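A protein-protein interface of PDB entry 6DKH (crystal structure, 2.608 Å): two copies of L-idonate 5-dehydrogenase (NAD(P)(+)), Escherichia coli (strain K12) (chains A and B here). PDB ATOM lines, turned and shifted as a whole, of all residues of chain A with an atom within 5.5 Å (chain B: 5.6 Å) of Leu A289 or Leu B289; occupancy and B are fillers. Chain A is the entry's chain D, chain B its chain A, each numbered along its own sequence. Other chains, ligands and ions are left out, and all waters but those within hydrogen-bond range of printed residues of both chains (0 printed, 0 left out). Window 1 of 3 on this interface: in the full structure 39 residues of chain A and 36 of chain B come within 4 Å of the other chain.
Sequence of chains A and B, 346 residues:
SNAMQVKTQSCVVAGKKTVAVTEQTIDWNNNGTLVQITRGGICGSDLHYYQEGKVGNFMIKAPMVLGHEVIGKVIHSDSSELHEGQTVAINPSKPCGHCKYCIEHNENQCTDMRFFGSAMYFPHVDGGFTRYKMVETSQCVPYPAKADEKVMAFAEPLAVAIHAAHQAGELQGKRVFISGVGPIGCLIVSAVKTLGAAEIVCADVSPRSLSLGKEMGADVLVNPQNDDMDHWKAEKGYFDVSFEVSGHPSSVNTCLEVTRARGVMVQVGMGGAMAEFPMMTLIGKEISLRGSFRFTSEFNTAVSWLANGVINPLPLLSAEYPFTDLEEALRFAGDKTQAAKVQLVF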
ATOM      1  N   GLY A 263       8.403  12.468 -25.693  1.00  0.00           N
ATOM      2  CA  GLY A 263       9.105  11.593 -26.604  1.00  0.00           C
ATOM      3  C   GLY A 263      10.079  10.689 -25.875  1.00  0.00           C
ATOM      4  O   GLY A 263      10.168  10.669 -24.648  1.00  0.00           O
ATOM      5  N   MET A 265      14.158   9.342 -25.734  1.00  0.00           N
ATOM      6  CA  MET A 265      15.552   9.615 -26.070  1.00  0.00           C
ATOM      7  C   MET A 265      16.400   8.457 -25.562  1.00  0.00           C
ATOM      8  O   MET A 265      16.532   8.266 -24.348  1.00  0.00           O
ATOM      9  CB  MET A 265      16.018  10.941 -25.470  1.00  0.00           C
ATOM     10  CG  MET A 265      17.516  11.165 -25.560  1.00  0.00           C
ATOM     11  SD  MET A 265      18.003  12.783 -24.942  1.00  0.00           S
ATOM     12  CE  MET A 265      19.697  12.457 -24.466  1.00  0.00           C
ATOM     13  N   VAL A 266      16.965   7.687 -26.486  1.00  0.00           N
ATOM     14  CA  VAL A 266      17.787   6.532 -26.145  1.00  0.00           C
ATOM     15  C   VAL A 266      19.240   6.977 -26.056  1.00  0.00           C
ATOM     16  O   VAL A 266      19.829   7.414 -27.051  1.00  0.00           O
ATOM     17  CB  VAL A 266      17.615   5.404 -27.172  1.00  0.00           C
ATOM     18  CG1 VAL A 266      18.617   4.291 -26.912  1.00  0.00           C
ATOM     19  CG2 VAL A 266      16.194   4.864 -27.126  1.00  0.00           C
ATOM     20  N   GLN A 267      19.818   6.865 -24.862  1.00  0.00           N
ATOM     21  CA  GLN A 267      21.199   7.262 -24.616  1.00  0.00           C
ATOM     22  C   GLN A 267      22.107   6.062 -24.866  1.00  0.00           C
ATOM     23  O   GLN A 267      22.087   5.090 -24.106  1.00  0.00           O
ATOM     24  CB  GLN A 267      21.357   7.790 -23.192  1.00  0.00           C
ATOM     25  CG  GLN A 267      22.780   8.157 -22.815  1.00  0.00           C
ATOM     26  CD  GLN A 267      23.314   9.338 -23.601  1.00  0.00           C
ATOM     27  OE1 GLN A 267      22.551  10.155 -24.116  1.00  0.00           O
ATOM     28  NE2 GLN A 267      24.637   9.435 -23.696  1.00  0.00           N
ATOM     29  N   PHE A 277      23.710  18.965 -16.931  1.00  0.00           N
ATOM     30  CA  PHE A 277      22.574  18.421 -17.663  1.00  0.00           C
ATOM     31  C   PHE A 277      21.349  19.312 -17.483  1.00  0.00           C
ATOM     32  O   PHE A 277      20.974  19.622 -16.345  1.00  0.00           O
ATOM     33  CB  PHE A 277      22.257  17.002 -17.193  1.00  0.00           C
ATOM     34  CG  PHE A 277      21.311  16.248 -18.107  1.00  0.00           C
ATOM     35  CD1 PHE A 277      21.603  16.083 -19.458  1.00  0.00           C
ATOM     36  CD2 PHE A 277      20.149  15.678 -17.613  1.00  0.00           C
ATOM     37  CE1 PHE A 277      20.738  15.377 -20.294  1.00  0.00           C
ATOM     38  CE2 PHE A 277      19.281  14.969 -18.447  1.00  0.00           C
ATOM     39  CZ  PHE A 277      19.580  14.821 -19.788  1.00  0.00           C
ATOM     40  N   MET A 279      18.342  19.313 -16.641  1.00  0.00           N
ATOM     41  CA  MET A 279      17.303  18.480 -16.045  1.00  0.00           C
ATOM     42  C   MET A 279      15.935  19.136 -16.166  1.00  0.00           C
ATOM     43  O   MET A 279      14.922  18.443 -16.293  1.00  0.00           O
ATOM     44  CB  MET A 279      17.639  18.193 -14.579  1.00  0.00           C
ATOM     45  CG  MET A 279      16.573  17.411 -13.822  1.00  0.00           C
ATOM     46  SD  MET A 279      16.183  15.826 -14.588  1.00  0.00           S
ATOM     47  CE  MET A 279      17.676  14.897 -14.250  1.00  0.00           C
ATOM     48  N   LEU A 282      14.278  18.104 -19.282  1.00  0.00           N
ATOM     49  CA  LEU A 282      13.749  16.747 -19.176  1.00  0.00           C
ATOM     50  C   LEU A 282      12.429  16.730 -18.415  1.00  0.00           C
ATOM     51  O   LEU A 282      11.481  16.044 -18.815  1.00  0.00           O
ATOM     52  CB  LEU A 282      14.781  15.840 -18.498  1.00  0.00           C
ATOM     53  CG  LEU A 282      14.391  14.393 -18.180  1.00  0.00           C
ATOM     54  CD1 LEU A 282      14.062  13.635 -19.445  1.00  0.00           C
ATOM     55  CD2 LEU A 282      15.507  13.694 -17.428  1.00  0.00           C
ATOM     56  N   ILE A 287      10.322  14.034 -21.205  1.00  0.00           N
ATOM     57  CA  ILE A 287      11.043  13.116 -22.078  1.00  0.00           C
ATOM     58  C   ILE A 287      11.329  11.822 -21.332  1.00  0.00           C
ATOM     59  O   ILE A 287      11.622  11.826 -20.128  1.00  0.00           O
ATOM     60  CB  ILE A 287      12.344  13.763 -22.585  1.00  0.00           C
ATOM     61  CG1 ILE A 287      12.051  15.094 -23.279  1.00  0.00           C
ATOM     62  CG2 ILE A 287      13.086  12.823 -23.525  1.00  0.00           C
ATOM     63  CD1 ILE A 287      11.203  14.954 -24.517  1.00  0.00           C
ATOM     64  N   SER A 288      11.234  10.702 -22.043  1.00  0.00           N
ATOM     65  CA  SER A 288      11.521   9.385 -21.477  1.00  0.00           C
ATOM     66  C   SER A 288      12.951   9.016 -21.865  1.00  0.00           C
ATOM     67  O   SER A 288      13.199   8.428 -22.917  1.00  0.00           O
ATOM     68  CB  SER A 288      10.509   8.357 -21.967  1.00  0.00           C
ATOM     69  OG  SER A 288      10.554   7.179 -21.182  1.00  0.00           O
ATOM     70  N   LEU A 289      13.901   9.379 -21.002  1.00  0.00           N
ATOM     71  CA  LEU A 289      15.311   9.085 -21.233  1.00  0.00           C
ATOM     72  C   LEU A 289      15.605   7.649 -20.819  1.00  0.00           C
ATOM     73  O   LEU A 289      15.458   7.293 -19.644  1.00  0.00           O
ATOM     74  CB  LEU A 289      16.192  10.062 -20.457  1.00  0.00           C
ATOM     75  CG  LEU A 289      17.698   9.795 -20.495  1.00  0.00           C
ATOM     76  CD1 LEU A 289      18.228   9.911 -21.916  1.00  0.00           C
ATOM     77  CD2 LEU A 289      18.438  10.740 -19.558  1.00  0.00           C
ATOM     78  N   ARG A 290      16.031   6.829 -21.776  1.00  0.00           N
ATOM     79  CA  ARG A 290      16.287   5.415 -21.548  1.00  0.00           C
ATOM     80  C   ARG A 290      17.706   5.081 -21.983  1.00  0.00           C
ATOM     81  O   ARG A 290      18.120   5.435 -23.092  1.00  0.00           O
ATOM     82  CB  ARG A 290      15.278   4.548 -22.305  1.00  0.00           C
ATOM     83  CG  ARG A 290      13.833   4.846 -21.946  1.00  0.00           C
ATOM     84  CD  ARG A 290      12.864   4.237 -22.942  1.00  0.00           C
ATOM     85  NE  ARG A 290      11.487   4.627 -22.654  1.00  0.00           N
ATOM     86  CZ  ARG A 290      10.437   4.274 -23.389  1.00  0.00           C
ATOM     87  NH1 ARG A 290       9.221   4.678 -23.049  1.00  0.00           N
ATOM     88  NH2 ARG A 290      10.605   3.519 -24.465  1.00  0.00           N
ATOM     89  N   GLY A 291      18.445   4.402 -21.106  1.00  0.00           N
ATOM     90  CA  GLY A 291      19.782   3.975 -21.447  1.00  0.00           C
ATOM     91  C   GLY A 291      19.799   2.649 -22.183  1.00  0.00           C
ATOM     92  O   GLY A 291      18.875   1.842 -22.098  1.00  0.00           O
ATOM     93  N   GLY B 263      15.047  -0.375 -14.309  1.00  0.00           N
ATOM     94  CA  GLY B 263      13.965   0.168 -13.521  1.00  0.00           C
ATOM     95  C   GLY B 263      13.497   1.508 -14.055  1.00  0.00           C
ATOM     96  O   GLY B 263      13.921   1.980 -15.111  1.00  0.00           O
ATOM     97  N   MET B 265      12.761   5.629 -13.036  1.00  0.00           N
ATOM     98  CA  MET B 265      13.039   6.750 -12.144  1.00  0.00           C
ATOM     99  C   MET B 265      12.209   7.938 -12.606  1.00  0.00           C
ATOM    100  O   MET B 265      12.462   8.498 -13.679  1.00  0.00           O
ATOM    101  CB  MET B 265      14.529   7.095 -12.129  1.00  0.00           C
ATOM    102  CG  MET B 265      14.875   8.306 -11.277  1.00  0.00           C
ATOM    103  SD  MET B 265      16.648   8.620 -11.180  1.00  0.00           S
ATOM    104  CE  MET B 265      16.674  10.166 -10.274  1.00  0.00           C
ATOM    105  N   VAL B 266      11.217   8.317 -11.806  1.00  0.00           N
ATOM    106  CA  VAL B 266      10.347   9.444 -12.123  1.00  0.00           C
ATOM    107  C   VAL B 266      10.927  10.696 -11.480  1.00  0.00           C
ATOM    108  O   VAL B 266      11.067  10.768 -10.253  1.00  0.00           O
ATOM    109  CB  VAL B 266       8.910   9.188 -11.645  1.00  0.00           C
ATOM    110  CG1 VAL B 266       8.034  10.398 -11.930  1.00  0.00           C
ATOM    111  CG2 VAL B 266       8.346   7.946 -12.314  1.00  0.00           C
ATOM    112  N   GLN B 267      11.262  11.682 -12.307  1.00  0.00           N
ATOM    113  CA  GLN B 267      11.866  12.929 -11.851  1.00  0.00           C
ATOM    114  C   GLN B 267      10.770  13.976 -11.688  1.00  0.00           C
ATOM    115  O   GLN B 267      10.143  14.384 -12.670  1.00  0.00           O
ATOM    116  CB  GLN B 267      12.934  13.401 -12.834  1.00  0.00           C
ATOM    117  CG  GLN B 267      13.604  14.699 -12.434  1.00  0.00           C
ATOM    118  CD  GLN B 267      14.525  14.540 -11.245  1.00  0.00           C
ATOM    119  OE1 GLN B 267      15.182  13.511 -11.088  1.00  0.00           O
ATOM    120  NE2 GLN B 267      14.579  15.561 -10.397  1.00  0.00           N
ATOM    121  N   PHE B 277      26.069  15.133 -13.645  1.00  0.00           N
ATOM    122  CA  PHE B 277      25.083  14.064 -13.762  1.00  0.00           C
ATOM    123  C   PHE B 277      25.766  12.753 -14.130  1.00  0.00           C
ATOM    124  O   PHE B 277      26.431  12.684 -15.172  1.00  0.00           O
ATOM    125  CB  PHE B 277      24.032  14.428 -14.807  1.00  0.00           C
ATOM    126  CG  PHE B 277      23.050  13.327 -15.091  1.00  0.00           C
ATOM    127  CD1 PHE B 277      22.064  13.005 -14.173  1.00  0.00           C
ATOM    128  CD2 PHE B 277      23.107  12.620 -16.281  1.00  0.00           C
ATOM    129  CE1 PHE B 277      21.159  11.993 -14.432  1.00  0.00           C
ATOM    130  CE2 PHE B 277      22.202  11.608 -16.547  1.00  0.00           C
ATOM    131  CZ  PHE B 277      21.228  11.294 -15.621  1.00  0.00           C
ATOM    132  N   MET B 279      25.712  10.117 -16.004  1.00  0.00           N
ATOM    133  CA  MET B 279      25.039   9.501 -17.142  1.00  0.00           C
ATOM    134  C   MET B 279      25.538   8.082 -17.384  1.00  0.00           C
ATOM    135  O   MET B 279      24.792   7.246 -17.907  1.00  0.00           O
ATOM    136  CB  MET B 279      25.226  10.369 -18.388  1.00  0.00           C
ATOM    137  CG  MET B 279      24.568   9.827 -19.648  1.00  0.00           C
ATOM    138  SD  MET B 279      24.183  11.118 -20.846  1.00  0.00           S
ATOM    139  CE  MET B 279      22.619  11.716 -20.207  1.00  0.00           C
ATOM    140  N   LEU B 282      23.260   5.667 -15.687  1.00  0.00           N
ATOM    141  CA  LEU B 282      21.990   5.472 -16.374  1.00  0.00           C
ATOM    142  C   LEU B 282      22.159   4.608 -17.618  1.00  0.00           C
ATOM    143  O   LEU B 282      21.244   3.863 -17.984  1.00  0.00           O
ATOM    144  CB  LEU B 282      21.377   6.829 -16.732  1.00  0.00           C
ATOM    145  CG  LEU B 282      19.916   6.884 -17.189  1.00  0.00           C
ATOM    146  CD1 LEU B 282      19.288   8.193 -16.749  1.00  0.00           C
ATOM    147  CD2 LEU B 282      19.797   6.731 -18.700  1.00  0.00           C
ATOM    148  N   ILE B 287      18.384   2.567 -16.905  1.00  0.00           N
ATOM    149  CA  ILE B 287      17.250   3.090 -16.156  1.00  0.00           C
ATOM    150  C   ILE B 287      16.418   3.991 -17.056  1.00  0.00           C
ATOM    151  O   ILE B 287      16.953   4.824 -17.802  1.00  0.00           O
ATOM    152  CB  ILE B 287      17.732   3.846 -14.906  1.00  0.00           C
ATOM    153  CG1 ILE B 287      18.551   2.920 -14.007  1.00  0.00           C
ATOM    154  CG2 ILE B 287      16.552   4.433 -14.144  1.00  0.00           C
ATOM    155  CD1 ILE B 287      19.926   3.456 -13.688  1.00  0.00           C
ATOM    156  N   SER B 288      15.099   3.823 -16.999  1.00  0.00           N
ATOM    157  CA  SER B 288      14.177   4.663 -17.758  1.00  0.00           C
ATOM    158  C   SER B 288      13.862   5.891 -16.912  1.00  0.00           C
ATOM    159  O   SER B 288      13.078   5.823 -15.963  1.00  0.00           O
ATOM    160  CB  SER B 288      12.917   3.888 -18.127  1.00  0.00           C
ATOM    161  OG  SER B 288      12.088   4.644 -18.990  1.00  0.00           O
ATOM    162  N   LEU B 289      14.487   7.017 -17.252  1.00  0.00           N
ATOM    163  CA  LEU B 289      14.331   8.267 -16.516  1.00  0.00           C
ATOM    164  C   LEU B 289      13.236   9.092 -17.182  1.00  0.00           C
ATOM    165  O   LEU B 289      13.430   9.621 -18.282  1.00  0.00           O
ATOM    166  CB  LEU B 289      15.651   9.034 -16.469  1.00  0.00           C
ATOM    167  CG  LEU B 289      15.653  10.399 -15.778  1.00  0.00           C
ATOM    168  CD1 LEU B 289      15.061  10.303 -14.383  1.00  0.00           C
ATOM    169  CD2 LEU B 289      17.065  10.961 -15.718  1.00  0.00           C
ATOM    170  N   ARG B 290      12.093   9.202 -16.514  1.00  0.00           N
ATOM    171  CA  ARG B 290      10.934   9.906 -17.040  1.00  0.00           C
ATOM    172  C   ARG B 290      10.679  11.171 -16.233  1.00  0.00           C
ATOM    173  O   ARG B 290      10.888  11.196 -15.016  1.00  0.00           O
ATOM    174  CB  ARG B 290       9.695   9.008 -17.012  1.00  0.00           C
ATOM    175  CG  ARG B 290       9.825   7.778 -17.889  1.00  0.00           C
ATOM    176  CD  ARG B 290       8.952   6.645 -17.390  1.00  0.00           C
ATOM    177  NE  ARG B 290       9.098   5.448 -18.210  1.00  0.00           N
ATOM    178  CZ  ARG B 290       8.524   4.281 -17.938  1.00  0.00           C
ATOM    179  NH1 ARG B 290       8.714   3.244 -18.742  1.00  0.00           N
ATOM    180  NH2 ARG B 290       7.763   4.149 -16.861  1.00  0.00           N
ATOM    181  N   GLY B 291      10.232  12.217 -16.918  1.00  0.00           N
ATOM    182  CA  GLY B 291       9.892  13.473 -16.281  1.00  0.00           C
ATOM    183  C   GLY B 291       8.399  13.585 -16.038  1.00  0.00           C
ATOM    184  O   GLY B 291       7.590  13.030 -16.777  1.00  0.00           O
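SD of Met B279 is in hydrogen-bond range of NE2 of Gln A267 (3.3 Å).
The backbone NH (N) of Leu B289 lies within hydrogen-bond range of the backbone carbonyl oxygen (O) of Leu A289, 2.6 Å away.
The backbone carbonyl oxygen of Ile A287 lies close to the backbone carbonyl oxygen of Leu B289 (3.4 Å).
The backbone carbonyl oxygen (O) of Leu A289 sits close to the backbone carbonyl oxygen (O) of Ile B287.
Hydrophobic or aromatic side chains of chain A within 4 Å of the printed part of chain B: Phe A277, Met A279, Leu A282 and Leu A289.
Of the 12 printed residues of chain B, 9 touch a printed residue of chain A.
Printed residues of chain B that touch a printed residue of chain A: Gln B267, Phe B277, Met B279, Leu B282, Ile B287, Ser B288, Leu B289, Arg B290 and Gly B291.
The backbone carbonyl oxygen (O) of Gly B263 sits at hydrogen-bond distance from the backbone NH (N) of Ser B288, 2.9 Å away.
The backbone NH (N) of Met B265 sits at hydrogen-bond distance from the backbone carbonyl oxygen (O) of Ser B288 (3.0 Å).
O of Arg B290 lies within hydrogen-bond range of N of Gln B267.
OG of Ser B288 lies within hydrogen-bond range of NE of Arg B290 (3.2 Å).
O of Gly A263 lies within hydrogen-bond range of N of Ser A288, 2.8 Å away.
O of Leu A282 lies within hydrogen-bond range of N of Ile A287, 3.3 Å away.
Among the printed residues, pairs that only touch across the chains: Phe A277 with Phe B277, Met A279 with Gln B267, Leu A282 with Leu B289, Leu A282 with Gly B291, Ile A287 with Arg B290, Ile A287 with Gly B291, Ser A288 with Ser B288, Ser A288 with Leu B289, Ser A288 with Arg B290, Leu A289 with Leu B282, Leu A289 with Ser B288, Arg A290 with Ile B287, Arg A290 with Ser B288, Gly A291 with Leu B282 and Gly A291 with Ile B287.
Of chain A, only Leu A282, Ile A287, Ser A288 and Leu A289 come within 4 Å of Leu B289.
Of the printed residues of chain B, Arg A290 touches Ile B287 (3.9 Å) and Ser B288 (3.4 Å).
Of the printed residues of chain A, Leu B282 touches Leu A289 (3.9 Å) and Gly A291 (3.6 Å).
Of the printed residues of chain B, Phe A277 touches Phe B277 (3.9 Å).
Gly A263 touches none of the printed residues of chain B.
Met A265 touches none of the printed residues of chain B.
The nearest residue of chain B that does not touch Leu A289 is Met B279 (4.3 Å).
The nearest residue of chain A that does not touch Leu B289 is Met A279 (4.2 Å).
Phe B277 touches its own counterpart, Phe A277.
Ile A287 touches Gly B291, and with the chains exchanged Gly A291 touches Ile B287.
Ser A288 touches Leu B289, and with the chains exchanged Leu A289 touches Ser B288.
Leu A289 touches its own counterpart, Leu B289.
Positions printed for both chains: 263, 265, 266, 267, 277, 279, 282, 287, 288, 289, 290 and 291.
Of the 19 pairs that touch across the chains among the printed residues, 19 have their exchanged pair printed and touching as well.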
